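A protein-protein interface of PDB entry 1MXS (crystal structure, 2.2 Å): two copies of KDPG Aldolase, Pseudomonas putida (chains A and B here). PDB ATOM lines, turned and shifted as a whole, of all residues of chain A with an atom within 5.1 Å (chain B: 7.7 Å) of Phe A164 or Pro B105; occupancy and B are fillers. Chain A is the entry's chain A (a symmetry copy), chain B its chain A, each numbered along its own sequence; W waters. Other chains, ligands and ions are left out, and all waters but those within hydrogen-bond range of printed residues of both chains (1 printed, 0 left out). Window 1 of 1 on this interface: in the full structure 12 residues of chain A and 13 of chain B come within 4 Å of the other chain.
The backbone NH (N) of Gly B106 sits close to the side-chain sulfur (SD) of Met A133 (3.5 Å).
The backbone NH (N) of Ile B107 is in hydrogen-bond range of the side-chain hydroxyl (OG) of Ser A130.
The guanidinium group of Arg B60 is in hydrogen-bond range of the side-chain hydroxyl of Thr B84 (3.1 Å).
N of Thr B84 lies within hydrogen-bond range of O of Val B103, at 3.3 Å.
O of Gly B106 lies within hydrogen-bond range of OG1 of Thr B104, 2.8 Å away.
The backbone carbonyl oxygen (O) of Thr B104 lies within hydrogen-bond range of the backbone NH (N) of Gly B125, 3.1 Å away.
The backbone NH (N) of Phe B146 lies within hydrogen-bond range of the backbone carbonyl oxygen (O) of Ile B126, 3.0 Å away.
OE2 of Glu B131 sits at hydrogen-bond distance from N of Ser B127 (2.9 Å).
Phe B146 touches Pro A129 (O to CG, 3.96 Å).
OG of Ser A130 touches O of Gly B125, 3.8 Å away.
Ser A130 touches Glu B131 (CB to OE1, 3.3 Å).
Met A133 touches Leu B86 (CE to CA, 3.7 Å).
CE of Met A133 touches CD1 of Ile B111 (3.2 Å).
Arg B60 touches Gly A162 (CD to O, 3.4 Å).
N of Pro A163 touches CZ of Arg B60, at 3.7 Å.
Pro A163 touches Pro B105.
Phe A164 touches Leu B86.
CZ of Phe A164 touches CG of Pro B105, 3.7 Å away.
Of the printed residues of chain B, Pro A129 touches Pro B105 (3.5 Å) and Phe B146 (3.96 Å).
Of the printed residues of chain B, Met A133 touches Val B85 (3.9 Å), Leu B86 (3.7 Å), Pro B105 (3.8 Å), Gly B106 (3.4 Å) and Ile B111 (3.2 Å).
Pro A163 touches just these residues of chain B: Arg B60 (3.7 Å), Thr B84 (3.7 Å) and Pro B105 (3.95 Å).
Of the printed residues of chain B, Phe A164 touches Leu B86 and Pro B105.
Gly B83 touches none of the printed residues of chain A.
Pro B105 touches four residues of chain A.
Printed residues of chain A within 4 Å of Gly B106: Ser A130 (3.3 Å) and Met A133 (3.4 Å).
Of the printed residues of chain A, Ile B111 touches Met A133.
Ile B126 touches none of the printed residues of chain A.
The nearest printed residue of chain B that does not touch Phe A164 is Phe B146 (5.2 Å).
The nearest residue of chain A that does not touch Pro B105 is Ser A130 (5.0 Å).
Printed residues of chain A that touch a printed residue of chain B: Pro A129, Ser A130, Met A133, Gly A162, Pro A163 and Phe A164.
Hydrophobic or aromatic side chains of chain A within 4 Å of the printed part of chain B: Pro A129, Met A133, Pro A163 and Phe A164.
Of the 22 printed residues of chain B, 11 touch a printed residue of chain A.
Hydrophobic or aromatic side chains of chain B that line the printed part of chain A: Leu B86, Pro B105, Ile B107, Ile B111 and Phe B146.
Among the printed residues, 17 pairs touch across the chains.
Among the printed residues, no Asp or Glu carboxylate lies within 4 Å of a Lys or Arg side-chain nitrogen of the other chain.
No position is printed for both chains.
Water W1 bridges the side-chain carboxylate (OE2) of Glu B131 (2.6 Å) and the backbone NH (N) of Ser A130 (3.1 Å).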
ATOM      1  N   PRO A 129      18.255 -28.155 -20.172  1.00  0.00           N
ATOM      2  CA  PRO A 129      19.610 -27.944 -20.690  1.00  0.00           C
ATOM      3  C   PRO A 129      20.686 -28.021 -19.591  1.00  0.00           C
ATOM      4  O   PRO A 129      21.776 -28.562 -19.809  1.00  0.00           O
ATOM      5  CB  PRO A 129      19.525 -26.553 -21.311  1.00  0.00           C
ATOM      6  CG  PRO A 129      18.124 -26.496 -21.795  1.00  0.00           C
ATOM      7  CD  PRO A 129      17.352 -27.091 -20.648  1.00  0.00           C
ATOM      8  N   SER A 130      20.390 -27.472 -18.413  1.00  0.00           N
ATOM      9  CA  SER A 130      21.352 -27.505 -17.309  1.00  0.00           C
ATOM     10  C   SER A 130      21.657 -28.947 -16.899  1.00  0.00           C
ATOM     11  O   SER A 130      22.809 -29.302 -16.657  1.00  0.00           O
ATOM     12  CB  SER A 130      20.812 -26.727 -16.104  1.00  0.00           C
ATOM     13  OG  SER A 130      20.942 -25.336 -16.302  1.00  0.00           O
ATOM     14  N   ILE A 132      21.365 -31.528 -18.793  1.00  0.00           N
ATOM     15  CA  ILE A 132      22.107 -32.152 -19.884  1.00  0.00           C
ATOM     16  C   ILE A 132      23.584 -31.830 -19.706  1.00  0.00           C
ATOM     17  O   ILE A 132      24.445 -32.713 -19.789  1.00  0.00           O
ATOM     18  CB  ILE A 132      21.635 -31.615 -21.247  1.00  0.00           C
ATOM     19  CG1 ILE A 132      20.253 -32.190 -21.561  1.00  0.00           C
ATOM     20  CG2 ILE A 132      22.654 -31.952 -22.335  1.00  0.00           C
ATOM     21  CD1 ILE A 132      19.616 -31.635 -22.795  1.00  0.00           C
ATOM     22  N   MET A 133      23.879 -30.560 -19.451  1.00  0.00           N
ATOM     23  CA  MET A 133      25.260 -30.146 -19.258  1.00  0.00           C
ATOM     24  C   MET A 133      25.923 -30.859 -18.086  1.00  0.00           C
ATOM     25  O   MET A 133      27.083 -31.250 -18.170  1.00  0.00           O
ATOM     26  CB  MET A 133      25.337 -28.633 -19.063  1.00  0.00           C
ATOM     27  CG  MET A 133      25.100 -27.872 -20.343  1.00  0.00           C
ATOM     28  SD  MET A 133      25.053 -26.120 -20.079  1.00  0.00           S
ATOM     29  CE  MET A 133      26.806 -25.764 -19.995  1.00  0.00           C
ATOM     30  N   PHE A 160      16.991 -28.463 -28.069  1.00  0.00           N
ATOM     31  CA  PHE A 160      18.254 -28.967 -27.522  1.00  0.00           C
ATOM     32  C   PHE A 160      19.262 -29.319 -28.600  1.00  0.00           C
ATOM     33  O   PHE A 160      20.467 -29.315 -28.354  1.00  0.00           O
ATOM     34  CB  PHE A 160      18.015 -30.197 -26.646  1.00  0.00           C
ATOM     35  CG  PHE A 160      17.089 -29.950 -25.498  1.00  0.00           C
ATOM     36  CD1 PHE A 160      17.030 -28.704 -24.883  1.00  0.00           C
ATOM     37  CD2 PHE A 160      16.278 -30.974 -25.017  1.00  0.00           C
ATOM     38  CE1 PHE A 160      16.175 -28.488 -23.803  1.00  0.00           C
ATOM     39  CE2 PHE A 160      15.424 -30.765 -23.939  1.00  0.00           C
ATOM     40  CZ  PHE A 160      15.367 -29.519 -23.328  1.00  0.00           C
ATOM     41  N   GLY A 161      18.767 -29.631 -29.792  1.00  0.00           N
ATOM     42  CA  GLY A 161      19.658 -29.982 -30.879  1.00  0.00           C
ATOM     43  C   GLY A 161      20.578 -28.844 -31.281  1.00  0.00           C
ATOM     44  O   GLY A 161      21.672 -29.074 -31.801  1.00  0.00           O
ATOM     45  N   GLY A 162      20.134 -27.613 -31.047  1.00  0.00           N
ATOM     46  CA  GLY A 162      20.932 -26.454 -31.398  1.00  0.00           C
ATOM     47  C   GLY A 162      22.244 -26.381 -30.636  1.00  0.00           C
ATOM     48  O   GLY A 162      23.320 -26.523 -31.235  1.00  0.00           O
ATOM     49  N   PRO A 163      22.196 -26.145 -29.315  1.00  0.00           N
ATOM     50  CA  PRO A 163      23.428 -26.065 -28.526  1.00  0.00           C
ATOM     51  C   PRO A 163      24.135 -27.408 -28.330  1.00  0.00           C
ATOM     52  O   PRO A 163      25.364 -27.461 -28.280  1.00  0.00           O
ATOM     53  CB  PRO A 163      22.954 -25.437 -27.219  1.00  0.00           C
ATOM     54  CG  PRO A 163      21.538 -25.893 -27.118  1.00  0.00           C
ATOM     55  CD  PRO A 163      21.040 -25.690 -28.525  1.00  0.00           C
ATOM     56  N   PHE A 164      23.358 -28.484 -28.223  1.00  0.00           N
ATOM     57  CA  PHE A 164      23.913 -29.822 -28.038  1.00  0.00           C
ATOM     58  C   PHE A 164      23.621 -30.645 -29.297  1.00  0.00           C
ATOM     59  O   PHE A 164      22.819 -31.577 -29.262  1.00  0.00           O
ATOM     60  CB  PHE A 164      23.274 -30.507 -26.814  1.00  0.00           C
ATOM     61  CG  PHE A 164      23.059 -29.593 -25.631  1.00  0.00           C
ATOM     62  CD1 PHE A 164      21.786 -29.096 -25.342  1.00  0.00           C
ATOM     63  CD2 PHE A 164      24.128 -29.216 -24.820  1.00  0.00           C
ATOM     64  CE1 PHE A 164      21.583 -28.230 -24.265  1.00  0.00           C
ATOM     65  CE2 PHE A 164      23.937 -28.349 -23.739  1.00  0.00           C
ATOM     66  CZ  PHE A 164      22.660 -27.855 -23.463  1.00  0.00           C
ATOM     67  N   GLY A 165      24.266 -30.294 -30.405  1.00  0.00           N
ATOM     68  CA  GLY A 165      24.027 -30.996 -31.655  1.00  0.00           C
ATOM     69  C   GLY A 165      24.619 -32.392 -31.766  1.00  0.00           C
ATOM     70  O   GLY A 165      24.314 -33.137 -32.706  1.00  0.00           O
ATOM     71  N   ASP A 166      25.462 -32.764 -30.808  1.00  0.00           N
ATOM     72  CA  ASP A 166      26.106 -34.074 -30.838  1.00  0.00           C
ATOM     73  C   ASP A 166      25.573 -35.107 -29.833  1.00  0.00           C
ATOM     74  O   ASP A 166      26.276 -36.060 -29.489  1.00  0.00           O
ATOM     75  CB  ASP A 166      27.621 -33.918 -30.654  1.00  0.00           C
ATOM     76  CG  ASP A 166      28.003 -33.403 -29.273  1.00  0.00           C
ATOM     77  OD1 ASP A 166      27.362 -32.432 -28.795  1.00  0.00           O
ATOM     78  OD2 ASP A 166      28.964 -33.954 -28.674  1.00  0.00           O
ATOM     79  N   ILE A 167      24.341 -34.924 -29.360  1.00  0.00           N
ATOM     80  CA  ILE A 167      23.746 -35.877 -28.425  1.00  0.00           C
ATOM     81  C   ILE A 167      22.427 -36.423 -28.961  1.00  0.00           C
ATOM     82  O   ILE A 167      21.708 -35.734 -29.675  1.00  0.00           O
ATOM     83  CB  ILE A 167      23.508 -35.247 -27.023  1.00  0.00           C
ATOM     84  CG1 ILE A 167      22.512 -34.106 -27.122  1.00  0.00           C
ATOM     85  CG2 ILE A 167      24.821 -34.724 -26.441  1.00  0.00           C
ATOM     86  CD1 ILE A 167      22.146 -33.501 -25.792  1.00  0.00           C
ATOM     87  N   GLU B  56      26.183 -12.396 -30.583  1.00  0.00           N
ATOM     88  CA  GLU B  56      26.518 -13.549 -29.759  1.00  0.00           C
ATOM     89  C   GLU B  56      27.003 -14.633 -30.707  1.00  0.00           C
ATOM     90  O   GLU B  56      26.201 -15.249 -31.409  1.00  0.00           O
ATOM     91  CB  GLU B  56      25.302 -14.061 -28.990  1.00  0.00           C
ATOM     92  CG  GLU B  56      25.682 -15.067 -27.916  1.00  0.00           C
ATOM     93  CD  GLU B  56      24.666 -16.183 -27.744  1.00  0.00           C
ATOM     94  OE1 GLU B  56      23.506 -15.885 -27.407  1.00  0.00           O
ATOM     95  OE2 GLU B  56      25.032 -17.361 -27.955  1.00  0.00           O
ATOM     96  N   ARG B  60      29.187 -23.308 -31.572  1.00  0.00           N
ATOM     97  CA  ARG B  60      28.531 -24.463 -32.179  1.00  0.00           C
ATOM     98  C   ARG B  60      29.240 -24.947 -33.434  1.00  0.00           C
ATOM     99  O   ARG B  60      28.880 -25.978 -33.986  1.00  0.00           O
ATOM    100  CB  ARG B  60      27.065 -24.142 -32.494  1.00  0.00           C
ATOM    101  CG  ARG B  60      26.257 -23.722 -31.273  1.00  0.00           C
ATOM    102  CD  ARG B  60      24.798 -23.464 -31.605  1.00  0.00           C
ATOM    103  NE  ARG B  60      24.096 -22.842 -30.484  1.00  0.00           N
ATOM    104  CZ  ARG B  60      22.785 -22.619 -30.447  1.00  0.00           C
ATOM    105  NH1 ARG B  60      22.239 -22.049 -29.385  1.00  0.00           N
ATOM    106  NH2 ARG B  60      22.014 -22.979 -31.467  1.00  0.00           N
ATOM    107  N   GLY B  83      28.972 -17.687 -27.099  1.00  0.00           N
ATOM    108  CA  GLY B  83      27.903 -18.518 -26.583  1.00  0.00           C
ATOM    109  C   GLY B  83      28.174 -20.002 -26.755  1.00  0.00           C
ATOM    110  O   GLY B  83      29.119 -20.404 -27.444  1.00  0.00           O
ATOM    111  N   THR B  84      27.328 -20.817 -26.130  1.00  0.00           N
ATOM    112  CA  THR B  84      27.436 -22.274 -26.176  1.00  0.00           C
ATOM    113  C   THR B  84      28.744 -22.748 -25.553  1.00  0.00           C
ATOM    114  O   THR B  84      29.407 -23.656 -26.064  1.00  0.00           O
ATOM    115  CB  THR B  84      27.330 -22.801 -27.619  1.00  0.00           C
ATOM    116  OG1 THR B  84      26.168 -22.241 -28.238  1.00  0.00           O
ATOM    117  CG2 THR B  84      27.185 -24.310 -27.623  1.00  0.00           C
ATOM    118  N   VAL B  85      29.113 -22.100 -24.452  1.00  0.00           N
ATOM    119  CA  VAL B  85      30.310 -22.444 -23.701  1.00  0.00           C
ATOM    120  C   VAL B  85      29.858 -23.517 -22.727  1.00  0.00           C
ATOM    121  O   VAL B  85      29.141 -23.226 -21.774  1.00  0.00           O
ATOM    122  CB  VAL B  85      30.835 -21.223 -22.936  1.00  0.00           C
ATOM    123  CG1 VAL B  85      31.844 -21.660 -21.884  1.00  0.00           C
ATOM    124  CG2 VAL B  85      31.475 -20.241 -23.905  1.00  0.00           C
ATOM    125  N   LEU B  86      30.270 -24.757 -22.974  1.00  0.00           N
ATOM    126  CA  LEU B  86      29.843 -25.875 -22.135  1.00  0.00           C
ATOM    127  C   LEU B  86      30.746 -26.261 -20.960  1.00  0.00           C
ATOM    128  O   LEU B  86      30.329 -27.038 -20.105  1.00  0.00           O
ATOM    129  CB  LEU B  86      29.606 -27.105 -23.002  1.00  0.00           C
ATOM    130  CG  LEU B  86      28.727 -26.885 -24.232  1.00  0.00           C
ATOM    131  CD1 LEU B  86      28.565 -28.215 -24.942  1.00  0.00           C
ATOM    132  CD2 LEU B  86      27.364 -26.315 -23.847  1.00  0.00           C
ATOM    133  N   VAL B 103      27.849 -16.403 -22.679  1.00  0.00           N
ATOM    134  CA  VAL B 103      26.481 -16.904 -22.572  1.00  0.00           C
ATOM    135  C   VAL B 103      26.499 -18.427 -22.631  1.00  0.00           C
ATOM    136  O   VAL B 103      27.310 -18.998 -23.359  1.00  0.00           O
ATOM    137  CB  VAL B 103      25.622 -16.406 -23.749  1.00  0.00           C
ATOM    138  CG1 VAL B 103      24.211 -16.932 -23.605  1.00  0.00           C
ATOM    139  CG2 VAL B 103      25.631 -14.879 -23.809  1.00  0.00           C
ATOM    140  N   THR B 104      25.617 -19.081 -21.871  1.00  0.00           N
ATOM    141  CA  THR B 104      25.511 -20.549 -21.860  1.00  0.00           C
ATOM    142  C   THR B 104      24.041 -20.974 -21.971  1.00  0.00           C
ATOM    143  O   THR B 104      23.139 -20.201 -21.619  1.00  0.00           O
ATOM    144  CB  THR B 104      26.057 -21.174 -20.544  1.00  0.00           C
ATOM    145  OG1 THR B 104      25.325 -20.646 -19.428  1.00  0.00           O
ATOM    146  CG2 THR B 104      27.543 -20.884 -20.373  1.00  0.00           C
ATOM    147  N   PRO B 105      23.785 -22.196 -22.484  1.00  0.00           N
ATOM    148  CA  PRO B 105      22.419 -22.718 -22.628  1.00  0.00           C
ATOM    149  C   PRO B 105      21.826 -23.182 -21.286  1.00  0.00           C
ATOM    150  O   PRO B 105      20.606 -23.238 -21.113  1.00  0.00           O
ATOM    151  CB  PRO B 105      22.596 -23.879 -23.602  1.00  0.00           C
ATOM    152  CG  PRO B 105      23.984 -24.356 -23.318  1.00  0.00           C
ATOM    153  CD  PRO B 105      24.747 -23.054 -23.205  1.00  0.00           C
ATOM    154  N   GLY B 106      22.713 -23.531 -20.356  1.00  0.00           N
ATOM    155  CA  GLY B 106      22.321 -24.001 -19.043  1.00  0.00           C
ATOM    156  C   GLY B 106      23.457 -23.763 -18.071  1.00  0.00           C
ATOM    157  O   GLY B 106      24.462 -23.150 -18.435  1.00  0.00           O
ATOM    158  N   ILE B 107      23.321 -24.251 -16.841  1.00  0.00           N
ATOM    159  CA  ILE B 107      24.362 -24.044 -15.833  1.00  0.00           C
ATOM    160  C   ILE B 107      24.893 -25.318 -15.167  1.00  0.00           C
ATOM    161  O   ILE B 107      24.245 -26.355 -15.158  1.00  0.00           O
ATOM    162  CB  ILE B 107      23.848 -23.155 -14.680  1.00  0.00           C
ATOM    163  CG1 ILE B 107      22.709 -23.896 -13.959  1.00  0.00           C
ATOM    164  CG2 ILE B 107      23.380 -21.805 -15.214  1.00  0.00           C
ATOM    165  CD1 ILE B 107      22.357 -23.332 -12.593  1.00  0.00           C
ATOM    166  N   ILE B 111      30.960 -24.035 -14.366  1.00  0.00           N
ATOM    167  CA  ILE B 111      30.705 -22.822 -15.119  1.00  0.00           C
ATOM    168  C   ILE B 111      30.362 -21.619 -14.250  1.00  0.00           C
ATOM    169  O   ILE B 111      30.895 -20.539 -14.466  1.00  0.00           O
ATOM    170  CB  ILE B 111      29.579 -23.051 -16.118  1.00  0.00           C
ATOM    171  CG1 ILE B 111      30.135 -23.796 -17.322  1.00  0.00           C
ATOM    172  CG2 ILE B 111      28.941 -21.729 -16.505  1.00  0.00           C
ATOM    173  CD1 ILE B 111      29.092 -24.166 -18.327  1.00  0.00           C
ATOM    174  N   LEU B 123      26.354 -14.482 -18.675  1.00  0.00           N
ATOM    175  CA  LEU B 123      24.900 -14.502 -18.614  1.00  0.00           C
ATOM    176  C   LEU B 123      24.568 -15.990 -18.704  1.00  0.00           C
ATOM    177  O   LEU B 123      24.565 -16.568 -19.786  1.00  0.00           O
ATOM    178  CB  LEU B 123      24.289 -13.757 -19.801  1.00  0.00           C
ATOM    179  CG  LEU B 123      22.758 -13.624 -19.822  1.00  0.00           C
ATOM    180  CD1 LEU B 123      22.302 -12.719 -18.680  1.00  0.00           C
ATOM    181  CD2 LEU B 123      22.317 -13.058 -21.158  1.00  0.00           C
ATOM    182  N   PRO B 124      24.318 -16.643 -17.560  1.00  0.00           N
ATOM    183  CA  PRO B 124      24.000 -18.073 -17.572  1.00  0.00           C
ATOM    184  C   PRO B 124      22.558 -18.390 -17.970  1.00  0.00           C
ATOM    185  O   PRO B 124      21.629 -17.639 -17.660  1.00  0.00           O
ATOM    186  CB  PRO B 124      24.334 -18.503 -16.147  1.00  0.00           C
ATOM    187  CG  PRO B 124      23.927 -17.311 -15.352  1.00  0.00           C
ATOM    188  CD  PRO B 124      24.413 -16.138 -16.179  1.00  0.00           C
ATOM    189  N   GLY B 125      22.380 -19.503 -18.675  1.00  0.00           N
ATOM    190  CA  GLY B 125      21.049 -19.890 -19.107  1.00  0.00           C
ATOM    191  C   GLY B 125      20.340 -20.805 -18.120  1.00  0.00           C
ATOM    192  O   GLY B 125      20.885 -21.826 -17.698  1.00  0.00           O
ATOM    193  N   ILE B 126      19.118 -20.447 -17.745  1.00  0.00           N
ATOM    194  CA  ILE B 126      18.360 -21.271 -16.818  1.00  0.00           C
ATOM    195  C   ILE B 126      16.948 -21.582 -17.319  1.00  0.00           C
ATOM    196  O   ILE B 126      16.439 -20.937 -18.236  1.00  0.00           O
ATOM    197  CB  ILE B 126      18.268 -20.627 -15.422  1.00  0.00           C
ATOM    198  CG1 ILE B 126      17.494 -19.311 -15.495  1.00  0.00           C
ATOM    199  CG2 ILE B 126      19.669 -20.488 -14.835  1.00  0.00           C
ATOM    200  CD1 ILE B 126      15.966 -19.491 -15.459  1.00  0.00           C
ATOM    201  N   SER B 127      16.305 -22.549 -16.675  1.00  0.00           N
ATOM    202  CA  SER B 127      14.975 -23.002 -17.066  1.00  0.00           C
ATOM    203  C   SER B 127      14.009 -23.099 -15.884  1.00  0.00           C
ATOM    204  O   SER B 127      12.809 -22.881 -16.039  1.00  0.00           O
ATOM    205  CB  SER B 127      15.130 -24.369 -17.741  1.00  0.00           C
ATOM    206  OG  SER B 127      13.912 -24.851 -18.219  1.00  0.00           O
ATOM    207  N   GLU B 131      17.429 -23.885 -10.593  1.00  0.00           N
ATOM    208  CA  GLU B 131      18.595 -23.484 -11.343  1.00  0.00           C
ATOM    209  C   GLU B 131      18.890 -22.009 -11.095  1.00  0.00           C
ATOM    210  O   GLU B 131      20.053 -21.600 -11.009  1.00  0.00           O
ATOM    211  CB  GLU B 131      18.357 -23.777 -12.818  1.00  0.00           C
ATOM    212  CG  GLU B 131      18.263 -25.284 -13.065  1.00  0.00           C
ATOM    213  CD  GLU B 131      17.854 -25.673 -14.471  1.00  0.00           C
ATOM    214  OE1 GLU B 131      17.844 -26.895 -14.759  1.00  0.00           O
ATOM    215  OE2 GLU B 131      17.550 -24.769 -15.276  1.00  0.00           O
ATOM    216  N   LYS B 144      19.484 -15.815 -18.411  1.00  0.00           N
ATOM    217  CA  LYS B 144      18.936 -16.075 -19.717  1.00  0.00           C
ATOM    218  C   LYS B 144      17.957 -17.242 -19.568  1.00  0.00           C
ATOM    219  O   LYS B 144      18.319 -18.289 -19.030  1.00  0.00           O
ATOM    220  CB  LYS B 144      20.049 -16.463 -20.685  1.00  0.00           C
ATOM    221  CG  LYS B 144      19.534 -17.137 -21.930  1.00  0.00           C
ATOM    222  CD  LYS B 144      20.664 -17.524 -22.859  1.00  0.00           C
ATOM    223  CE  LYS B 144      20.120 -18.320 -24.026  1.00  0.00           C
ATOM    224  NZ  LYS B 144      21.106 -18.473 -25.126  1.00  0.00           N
ATOM    225  N   LEU B 145      16.728 -17.057 -20.045  1.00  0.00           N
ATOM    226  CA  LEU B 145      15.703 -18.099 -19.982  1.00  0.00           C
ATOM    227  C   LEU B 145      15.782 -18.908 -21.273  1.00  0.00           C
ATOM    228  O   LEU B 145      15.588 -18.364 -22.362  1.00  0.00           O
ATOM    229  CB  LEU B 145      14.314 -17.474 -19.857  1.00  0.00           C
ATOM    230  CG  LEU B 145      13.126 -18.427 -19.740  1.00  0.00           C
ATOM    231  CD1 LEU B 145      13.279 -19.246 -18.473  1.00  0.00           C
ATOM    232  CD2 LEU B 145      11.824 -17.642 -19.708  1.00  0.00           C
ATOM    233  N   PHE B 146      16.075 -20.202 -21.163  1.00  0.00           N
ATOM    234  CA  PHE B 146      16.175 -21.046 -22.355  1.00  0.00           C
ATOM    235  C   PHE B 146      15.762 -22.492 -22.070  1.00  0.00           C
ATOM    236  O   PHE B 146      16.235 -23.082 -21.096  1.00  0.00           O
ATOM    237  CB  PHE B 146      17.609 -21.018 -22.887  1.00  0.00           C
ATOM    238  CG  PHE B 146      17.831 -21.930 -24.059  1.00  0.00           C
ATOM    239  CD1 PHE B 146      17.272 -21.639 -25.300  1.00  0.00           C
ATOM    240  CD2 PHE B 146      18.532 -23.127 -23.904  1.00  0.00           C
ATOM    241  CE1 PHE B 146      17.404 -22.535 -26.369  1.00  0.00           C
ATOM    242  CE2 PHE B 146      18.666 -24.023 -24.960  1.00  0.00           C
ATOM    243  CZ  PHE B 146      18.103 -23.730 -26.194  1.00  0.00           C
ATOM    244  N   PRO B 147      14.848 -23.066 -22.890  1.00  0.00           N
ATOM    245  CA  PRO B 147      14.216 -22.403 -24.037  1.00  0.00           C
ATOM    246  C   PRO B 147      13.040 -21.587 -23.529  1.00  0.00           C
ATOM    247  O   PRO B 147      12.225 -22.089 -22.761  1.00  0.00           O
ATOM    248  CB  PRO B 147      13.735 -23.562 -24.906  1.00  0.00           C
ATOM    249  CG  PRO B 147      14.503 -24.751 -24.407  1.00  0.00           C
ATOM    250  CD  PRO B 147      14.582 -24.513 -22.935  1.00  0.00           C
HETATM  251  O   HOH W   1      18.215 -25.421 -17.732  1.00  0.00           O
